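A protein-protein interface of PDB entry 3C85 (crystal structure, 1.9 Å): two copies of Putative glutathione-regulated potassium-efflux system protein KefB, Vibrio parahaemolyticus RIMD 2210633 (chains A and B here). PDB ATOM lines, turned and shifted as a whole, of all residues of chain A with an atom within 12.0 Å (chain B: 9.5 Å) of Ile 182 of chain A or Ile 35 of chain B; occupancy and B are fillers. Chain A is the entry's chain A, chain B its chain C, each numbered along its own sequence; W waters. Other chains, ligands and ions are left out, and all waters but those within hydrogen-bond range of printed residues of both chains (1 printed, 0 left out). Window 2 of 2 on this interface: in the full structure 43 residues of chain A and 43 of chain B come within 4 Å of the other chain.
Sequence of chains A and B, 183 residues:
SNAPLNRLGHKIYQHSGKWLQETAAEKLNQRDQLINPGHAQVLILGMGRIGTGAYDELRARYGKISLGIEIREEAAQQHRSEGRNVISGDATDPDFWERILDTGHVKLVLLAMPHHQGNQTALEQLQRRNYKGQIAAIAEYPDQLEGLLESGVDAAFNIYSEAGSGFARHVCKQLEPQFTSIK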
ATOM      1  N   PRO A 177     -25.631   3.139  20.008  1.00  0.00           N
ATOM      2  CA  PRO A 177     -25.343   2.296  18.854  1.00  0.00           C
ATOM      3  C   PRO A 177     -25.027   0.859  19.303  1.00  0.00           C
ATOM      4  O   PRO A 177     -24.475   0.650  20.399  1.00  0.00           O
ATOM      5  CB  PRO A 177     -24.143   2.996  18.207  1.00  0.00           C
ATOM      6  CG  PRO A 177     -23.498   3.758  19.365  1.00  0.00           C
ATOM      7  CD  PRO A 177     -24.615   4.195  20.213  1.00  0.00           C
ATOM      8  N   GLN A 178     -25.393  -0.112  18.472  1.00  0.00           N
ATOM      9  CA  GLN A 178     -25.164  -1.508  18.803  1.00  0.00           C
ATOM     10  C   GLN A 178     -23.922  -2.036  18.086  1.00  0.00           C
ATOM     11  O   GLN A 178     -24.009  -2.490  16.969  1.00  0.00           O
ATOM     12  CB  GLN A 178     -26.400  -2.347  18.456  1.00  0.00           C
ATOM     13  CG  GLN A 178     -27.635  -2.026  19.342  1.00  0.00           C
ATOM     14  CD  GLN A 178     -28.585  -3.212  19.502  1.00  0.00           C
ATOM     15  OE1 GLN A 178     -29.419  -3.227  20.407  1.00  0.00           O
ATOM     16  NE2 GLN A 178     -28.453  -4.216  18.626  1.00  0.00           N
ATOM     17  N   PHE A 179     -22.769  -1.986  18.747  1.00  0.00           N
ATOM     18  CA  PHE A 179     -21.518  -2.420  18.142  1.00  0.00           C
ATOM     19  C   PHE A 179     -21.099  -3.813  18.586  1.00  0.00           C
ATOM     20  O   PHE A 179     -21.513  -4.287  19.651  1.00  0.00           O
ATOM     21  CB  PHE A 179     -20.383  -1.489  18.540  1.00  0.00           C
ATOM     22  CG  PHE A 179     -20.551  -0.085  18.083  1.00  0.00           C
ATOM     23  CD1 PHE A 179     -20.410   0.936  18.989  1.00  0.00           C
ATOM     24  CD2 PHE A 179     -20.810   0.209  16.754  1.00  0.00           C
ATOM     25  CE1 PHE A 179     -20.513   2.258  18.607  1.00  0.00           C
ATOM     26  CE2 PHE A 179     -20.939   1.528  16.347  1.00  0.00           C
ATOM     27  CZ  PHE A 179     -20.790   2.564  17.294  1.00  0.00           C
ATOM     28  N   THR A 180     -20.267  -4.458  17.780  1.00  0.00           N
ATOM     29  CA  THR A 180     -19.552  -5.646  18.237  1.00  0.00           C
ATOM     30  C   THR A 180     -18.200  -5.183  18.768  1.00  0.00           C
ATOM     31  O   THR A 180     -17.335  -4.797  17.987  1.00  0.00           O
ATOM     32  CB  THR A 180     -19.354  -6.666  17.102  1.00  0.00           C
ATOM     33  OG1 THR A 180     -20.622  -6.951  16.500  1.00  0.00           O
ATOM     34  CG2 THR A 180     -18.744  -7.975  17.653  1.00  0.00           C
ATOM     35  N   SER A 181     -18.032  -5.204  20.093  1.00  0.00           N
ATOM     36  CA  SER A 181     -16.798  -4.726  20.758  1.00  0.00           C
ATOM     37  C   SER A 181     -15.613  -5.649  20.512  1.00  0.00           C
ATOM     38  O   SER A 181     -15.737  -6.870  20.652  1.00  0.00           O
ATOM     39  CB  SER A 181     -17.002  -4.576  22.270  1.00  0.00           C
ATOM     40  OG  SER A 181     -17.847  -3.473  22.601  1.00  0.00           O
ATOM     41  N   ILE A 182     -14.463  -5.061  20.177  1.00  0.00           N
ATOM     42  CA  ILE A 182     -13.265  -5.828  19.830  1.00  0.00           C
ATOM     43  C   ILE A 182     -12.090  -5.413  20.730  1.00  0.00           C
ATOM     44  O   ILE A 182     -11.335  -4.500  20.395  1.00  0.00           O
ATOM     45  CB  ILE A 182     -12.881  -5.633  18.336  1.00  0.00           C
ATOM     46  CG1 ILE A 182     -14.082  -5.910  17.411  1.00  0.00           C
ATOM     47  CG2 ILE A 182     -11.619  -6.450  17.966  1.00  0.00           C
ATOM     48  CD1 ILE A 182     -14.692  -7.297  17.519  1.00  0.00           C
ATOM     49  N   LEU B  34      -9.135  -4.003  14.664  1.00  0.00           N
ATOM     50  CA  LEU B  34      -8.591  -4.307  13.317  1.00  0.00           C
ATOM     51  C   LEU B  34      -8.412  -5.835  13.120  1.00  0.00           C
ATOM     52  O   LEU B  34      -7.613  -6.272  12.298  1.00  0.00           O
ATOM     53  CB  LEU B  34      -7.294  -3.501  13.116  1.00  0.00           C
ATOM     54  CG  LEU B  34      -6.478  -3.504  11.813  1.00  0.00           C
ATOM     55  CD1 LEU B  34      -7.193  -2.836  10.624  1.00  0.00           C
ATOM     56  CD2 LEU B  34      -5.093  -2.863  12.058  1.00  0.00           C
ATOM     57  N   ILE B  35      -9.180  -6.639  13.866  1.00  0.00           N
ATOM     58  CA  ILE B  35      -9.165  -8.113  13.714  1.00  0.00           C
ATOM     59  C   ILE B  35      -9.464  -8.494  12.270  1.00  0.00           C
ATOM     60  O   ILE B  35      -8.799  -9.373  11.675  1.00  0.00           O
ATOM     61  CB  ILE B  35     -10.201  -8.812  14.631  1.00  0.00           C
ATOM     62  CG1 ILE B  35      -9.601  -9.008  16.031  1.00  0.00           C
ATOM     63  CG2 ILE B  35     -10.697 -10.153  13.992  1.00  0.00           C
ATOM     64  CD1 ILE B  35     -10.567  -9.598  17.067  1.00  0.00           C
ATOM     65  N   ASN B  36     -10.490  -7.836  11.735  1.00  0.00           N
ATOM     66  CA  ASN B  36     -10.823  -7.958  10.345  1.00  0.00           C
ATOM     67  C   ASN B  36     -10.685  -6.565   9.706  1.00  0.00           C
ATOM     68  O   ASN B  36     -11.544  -5.676   9.902  1.00  0.00           O
ATOM     69  CB  ASN B  36     -12.226  -8.547  10.180  1.00  0.00           C
ATOM     70  CG  ASN B  36     -12.421  -9.213   8.821  1.00  0.00           C
ATOM     71  OD1 ASN B  36     -11.597  -9.063   7.912  1.00  0.00           O
ATOM     72  ND2 ASN B  36     -13.519  -9.950   8.677  1.00  0.00           N
ATOM     73  N   PRO B  37      -9.576  -6.353   8.975  1.00  0.00           N
ATOM     74  CA  PRO B  37      -9.400  -5.070   8.330  1.00  0.00           C
ATOM     75  C   PRO B  37     -10.590  -4.830   7.409  1.00  0.00           C
ATOM     76  O   PRO B  37     -11.152  -5.782   6.876  1.00  0.00           O
ATOM     77  CB  PRO B  37      -8.101  -5.256   7.535  1.00  0.00           C
ATOM     78  CG  PRO B  37      -7.356  -6.348   8.281  1.00  0.00           C
ATOM     79  CD  PRO B  37      -8.462  -7.282   8.674  1.00  0.00           C
ATOM     80  N   GLY B  38     -11.000  -3.577   7.263  1.00  0.00           N
ATOM     81  CA  GLY B  38     -12.063  -3.255   6.326  1.00  0.00           C
ATOM     82  C   GLY B  38     -13.422  -3.357   6.971  1.00  0.00           C
ATOM     83  O   GLY B  38     -14.417  -2.975   6.369  1.00  0.00           O
ATOM     84  N   HIS B  39     -13.455  -3.812   8.231  1.00  0.00           N
ATOM     85  CA  HIS B  39     -14.718  -4.061   8.889  1.00  0.00           C
ATOM     86  C   HIS B  39     -15.029  -3.075   9.990  1.00  0.00           C
ATOM     87  O   HIS B  39     -15.871  -3.339  10.847  1.00  0.00           O
ATOM     88  CB  HIS B  39     -14.803  -5.531   9.355  1.00  0.00           C
ATOM     89  CG  HIS B  39     -14.951  -6.506   8.221  1.00  0.00           C
ATOM     90  ND1 HIS B  39     -16.105  -7.237   8.005  1.00  0.00           N
ATOM     91  CD2 HIS B  39     -14.119  -6.811   7.198  1.00  0.00           C
ATOM     92  CE1 HIS B  39     -15.961  -7.983   6.927  1.00  0.00           C
ATOM     93  NE2 HIS B  39     -14.767  -7.733   6.409  1.00  0.00           N
ATOM     94  N   ALA B  40     -14.386  -1.907   9.963  1.00  0.00           N
ATOM     95  CA  ALA B  40     -14.729  -0.868  10.959  1.00  0.00           C
ATOM     96  C   ALA B  40     -16.243  -0.547  10.996  1.00  0.00           C
ATOM     97  O   ALA B  40     -16.897  -0.373   9.946  1.00  0.00           O
ATOM     98  CB  ALA B  40     -13.926   0.388  10.729  1.00  0.00           C
ATOM     99  N   GLN B  41     -16.777  -0.457  12.211  1.00  0.00           N
ATOM    100  CA  GLN B  41     -18.171  -0.101  12.400  1.00  0.00           C
ATOM    101  C   GLN B  41     -18.379   1.392  12.613  1.00  0.00           C
ATOM    102  O   GLN B  41     -19.519   1.860  12.512  1.00  0.00           O
ATOM    103  CB  GLN B  41     -18.803  -0.868  13.550  1.00  0.00           C
ATOM    104  CG  GLN B  41     -18.689  -2.383  13.401  1.00  0.00           C
ATOM    105  CD  GLN B  41     -18.807  -3.088  14.709  1.00  0.00           C
ATOM    106  OE1 GLN B  41     -17.833  -3.616  15.241  1.00  0.00           O
ATOM    107  NE2 GLN B  41     -19.999  -3.116  15.244  1.00  0.00           N
ATOM    108  N   LEU B  58     -13.872   6.192  22.018  1.00  0.00           N
ATOM    109  CA  LEU B  58     -14.498   5.010  21.468  1.00  0.00           C
ATOM    110  C   LEU B  58     -13.612   3.774  21.647  1.00  0.00           C
ATOM    111  O   LEU B  58     -14.123   2.702  21.972  1.00  0.00           O
ATOM    112  CB  LEU B  58     -14.875   5.221  19.991  1.00  0.00           C
ATOM    113  CG  LEU B  58     -15.974   6.263  19.708  1.00  0.00           C
ATOM    114  CD1 LEU B  58     -16.091   6.519  18.203  1.00  0.00           C
ATOM    115  CD2 LEU B  58     -17.345   5.854  20.261  1.00  0.00           C
ATOM    116  N   ARG B  59     -12.319   3.911  21.482  1.00  0.00           N
ATOM    117  CA  ARG B  59     -11.433   2.794  21.672  1.00  0.00           C
ATOM    118  C   ARG B  59     -11.512   2.308  23.111  1.00  0.00           C
ATOM    119  O   ARG B  59     -11.568   1.148  23.340  1.00  0.00           O
ATOM    120  CB  ARG B  59      -9.999   3.097  21.306  1.00  0.00           C
ATOM    121  CG  ARG B  59      -9.025   2.135  21.919  1.00  0.00           C
ATOM    122  CD  ARG B  59      -7.953   1.723  21.047  1.00  0.00           C
ATOM    123  NE  ARG B  59      -6.905   0.984  21.740  1.00  0.00           N
ATOM    124  CZ  ARG B  59      -6.945  -0.300  22.119  1.00  0.00           C
ATOM    125  NH1 ARG B  59      -5.912  -0.839  22.719  1.00  0.00           N
ATOM    126  NH2 ARG B  59      -7.990  -1.059  21.917  1.00  0.00           N
ATOM    127  N   ALA B  60     -11.526   3.234  24.054  1.00  0.00           N
ATOM    128  CA  ALA B  60     -11.610   2.908  25.489  1.00  0.00           C
ATOM    129  C   ALA B  60     -12.853   2.086  25.802  1.00  0.00           C
ATOM    130  O   ALA B  60     -12.783   1.134  26.588  1.00  0.00           O
ATOM    131  CB  ALA B  60     -11.580   4.177  26.346  1.00  0.00           C
ATOM    132  N   ARG B  61     -13.975   2.438  25.168  1.00  0.00           N
ATOM    133  CA  ARG B  61     -15.229   1.764  25.436  1.00  0.00           C
ATOM    134  C   ARG B  61     -15.396   0.476  24.627  1.00  0.00           C
ATOM    135  O   ARG B  61     -15.814  -0.525  25.168  1.00  0.00           O
ATOM    136  CB  ARG B  61     -16.413   2.708  25.171  1.00  0.00           C
ATOM    137  CG  ARG B  61     -17.780   2.065  25.528  1.00  0.00           C
ATOM    138  CD  ARG B  61     -18.910   3.076  25.634  1.00  0.00           C
ATOM    139  NE  ARG B  61     -20.180   2.361  25.750  1.00  0.00           N
ATOM    140  CZ  ARG B  61     -21.365   2.923  25.954  1.00  0.00           C
ATOM    141  NH1 ARG B  61     -21.476   4.244  26.094  1.00  0.00           N
ATOM    142  NH2 ARG B  61     -22.444   2.149  26.030  1.00  0.00           N
ATOM    143  N   TYR B  62     -15.106   0.514  23.327  1.00  0.00           N
ATOM    144  CA  TYR B  62     -15.444  -0.613  22.445  1.00  0.00           C
ATOM    145  C   TYR B  62     -14.277  -1.411  21.871  1.00  0.00           C
ATOM    146  O   TYR B  62     -14.485  -2.409  21.157  1.00  0.00           O
ATOM    147  CB  TYR B  62     -16.301  -0.128  21.285  1.00  0.00           C
ATOM    148  CG  TYR B  62     -17.546   0.589  21.671  1.00  0.00           C
ATOM    149  CD1 TYR B  62     -18.678  -0.113  22.091  1.00  0.00           C
ATOM    150  CD2 TYR B  62     -17.606   1.990  21.615  1.00  0.00           C
ATOM    151  CE1 TYR B  62     -19.842   0.548  22.450  1.00  0.00           C
ATOM    152  CE2 TYR B  62     -18.758   2.663  21.970  1.00  0.00           C
ATOM    153  CZ  TYR B  62     -19.883   1.931  22.366  1.00  0.00           C
ATOM    154  OH  TYR B  62     -21.027   2.602  22.712  1.00  0.00           O
ATOM    155  N   GLY B  63     -13.060  -0.976  22.145  1.00  0.00           N
ATOM    156  CA  GLY B  63     -11.925  -1.540  21.450  1.00  0.00           C
ATOM    157  C   GLY B  63     -11.815  -1.075  20.004  1.00  0.00           C
ATOM    158  O   GLY B  63     -12.262   0.001  19.659  1.00  0.00           O
ATOM    159  N   LYS B  64     -11.224  -1.909  19.156  1.00  0.00           N
ATOM    160  CA  LYS B  64     -10.688  -1.415  17.909  1.00  0.00           C
ATOM    161  C   LYS B  64     -11.741  -1.569  16.804  1.00  0.00           C
ATOM    162  O   LYS B  64     -11.610  -2.406  15.912  1.00  0.00           O
ATOM    163  CB  LYS B  64      -9.303  -2.058  17.581  1.00  0.00           C
ATOM    164  CG  LYS B  64      -8.111  -1.555  18.504  1.00  0.00           C
ATOM    165  CD  LYS B  64      -6.691  -1.602  17.842  1.00  0.00           C
ATOM    166  CE  LYS B  64      -6.444  -0.354  16.960  1.00  0.00           C
ATOM    167  NZ  LYS B  64      -5.259  -0.368  16.052  1.00  0.00           N
ATOM    168  N   ILE B  65     -12.790  -0.749  16.883  1.00  0.00           N
ATOM    169  CA  ILE B  65     -13.907  -0.819  15.941  1.00  0.00           C
ATOM    170  C   ILE B  65     -14.016   0.421  15.033  1.00  0.00           C
ATOM    171  O   ILE B  65     -14.928   0.510  14.216  1.00  0.00           O
ATOM    172  CB  ILE B  65     -15.242  -1.050  16.699  1.00  0.00           C
ATOM    173  CG1 ILE B  65     -15.582   0.170  17.561  1.00  0.00           C
ATOM    174  CG2 ILE B  65     -15.125  -2.307  17.569  1.00  0.00           C
ATOM    175  CD1 ILE B  65     -17.056   0.347  17.914  1.00  0.00           C
ATOM    176  N   SER B  66     -13.078   1.348  15.168  1.00  0.00           N
ATOM    177  CA  SER B  66     -13.131   2.646  14.473  1.00  0.00           C
ATOM    178  C   SER B  66     -12.055   2.784  13.400  1.00  0.00           C
ATOM    179  O   SER B  66     -10.959   2.212  13.517  1.00  0.00           O
ATOM    180  CB  SER B  66     -13.001   3.811  15.474  1.00  0.00           C
ATOM    181  OG  SER B  66     -14.104   3.865  16.385  1.00  0.00           O
ATOM    182  N   ASN B  85      -5.873   3.529  14.063  1.00  0.00           N
ATOM    183  CA  ASN B  85      -6.338   2.997  12.790  1.00  0.00           C
ATOM    184  C   ASN B  85      -6.860   4.153  11.967  1.00  0.00           C
ATOM    185  O   ASN B  85      -8.027   4.514  12.111  1.00  0.00           O
ATOM    186  CB  ASN B  85      -7.487   1.997  12.983  1.00  0.00           C
ATOM    187  CG  ASN B  85      -7.871   1.289  11.682  1.00  0.00           C
ATOM    188  OD1 ASN B  85      -7.023   1.034  10.806  1.00  0.00           O
ATOM    189  ND2 ASN B  85      -9.148   0.975  11.539  1.00  0.00           N
ATOM    190  N   LYS B 107     -21.736   1.447  11.019  1.00  0.00           N
ATOM    191  CA  LYS B 107     -22.961   1.659  11.798  1.00  0.00           C
ATOM    192  C   LYS B 107     -23.089   3.077  12.264  1.00  0.00           C
ATOM    193  O   LYS B 107     -24.186   3.533  12.557  1.00  0.00           O
ATOM    194  CB  LYS B 107     -22.996   0.722  13.006  1.00  0.00           C
ATOM    195  CG  LYS B 107     -23.008  -0.753  12.541  1.00  0.00           C
ATOM    196  CD  LYS B 107     -23.065  -1.713  13.678  1.00  0.00           C
ATOM    197  CE  LYS B 107     -22.926  -3.127  13.164  1.00  0.00           C
ATOM    198  NZ  LYS B 107     -22.574  -4.038  14.279  1.00  0.00           N
HETATM  199  O   HOH W   1     -23.547   1.657  22.624  1.00  0.00           O
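Of chain B, only Ile 35, Tyr 62, Gly 63, Lys 64 and Ile 65 come within 4 Å of Ile 182 of chain A.
Printed residues of chain A within 4 Å of Ile 35 of chain B: Ile 182.
No residue of chain A comes within 4 Å of Leu 34 of chain B.
No residue of chain A comes within 4 Å of Asn 36 of chain B.
Of chain A, only Ile 182 comes within 4 Å of Lys 64 of chain B.
Ile 65 of chain B touches three residues of chain A.
Printed residues of chain B within 4 Å of Thr 180 of chain A: Gln 41 (2.9 Å) and Ile 65 (3.4 Å).
Of the printed residues of chain B, Gln 178 of chain A touches Lys 107.
Ala 40 of chain B touches none of the printed residues of chain A.
Arg 61 of chain B touches none of the printed residues of chain A.
The nearest residue of chain B that does not touch Ile 182 of chain A is Leu 34 of chain B (4.8 Å).
The nearest residue of chain A that does not touch Ile 35 of chain B is Ser 181 of chain A (6.9 Å).
The nearest printed residue of chain B that does not touch Gln 178 of chain A is Gln 41 of chain B (4.4 Å).
Gln 41 of chain B touches Phe 179 of chain A (NE2 to CA, 3.3 Å).
CD1 of Phe 179 of chain A touches CE1 of Tyr 62 of chain B (3.5 Å).
CG of Phe 179 of chain A touches CD1 of Ile 65 of chain B, 3.5 Å away.
CG2 of Ile 65 of chain B touches O of Thr 180 of chain A (3.4 Å).
O of Tyr 62 of chain B touches CA of Ser 181 of chain A, 3.3 Å away.
CG2 of Ile 182 of chain A touches CD1 of Ile 35 of chain B, 3.4 Å away.
O of Ile 182 of chain A touches CA of Gly 63 of chain B, 3.2 Å away.
CG2 of Ile 65 of chain B touches CG1 of Ile 182 of chain A, at 3.8 Å.
The backbone carbonyl oxygen of Ile 182 of chain A is in hydrogen-bond range of the backbone NH of Lys 64 of chain B.
The backbone NH of Thr 180 of chain A lies close to the side-chain amide nitrogen of Gln 41 of chain B.
The backbone carbonyl oxygen (O) of Gln 178 of chain A sits at hydrogen-bond distance from the side-chain amino group (NZ) of Lys 107 of chain B, at 3.4 Å.
The backbone NH (N) of Ile 182 of chain A lies within hydrogen-bond range of the backbone carbonyl oxygen (O) of Tyr 62 of chain B (2.8 Å).
No position is printed for both chains.
Of the 12 pairs that touch across the chains among the printed residues, none has its exchanged pair printed and touching as well.
Water W1 lies within hydrogen-bond range of the backbone carbonyl oxygen (O) of Pro 177 of chain A and the side-chain hydroxyl (OH) of Tyr 62 of chain B.
Hydrophobic or aromatic side chains of chain B within 4 Å of the printed part of chain A: Ile 35, Tyr 62 and Ile 65.
Among the printed residues, no Asp or Glu carboxylate lies within 4 Å of a Lys or Arg side-chain nitrogen of the other chain.
N of Lys 107 of chain B lies within hydrogen-bond range of O of Gln 41 of chain B (2.7 Å).
O of Lys 64 of chain B lies within hydrogen-bond range of N of Leu 34 of chain B.
O of Ile 65 of chain B lies within hydrogen-bond range of N of Gln 41 of chain B.
The guanidinium group (NE) of Arg 61 of chain B sits at hydrogen-bond distance from the side-chain hydroxyl (OH) of Tyr 62 of chain B (3.2 Å).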
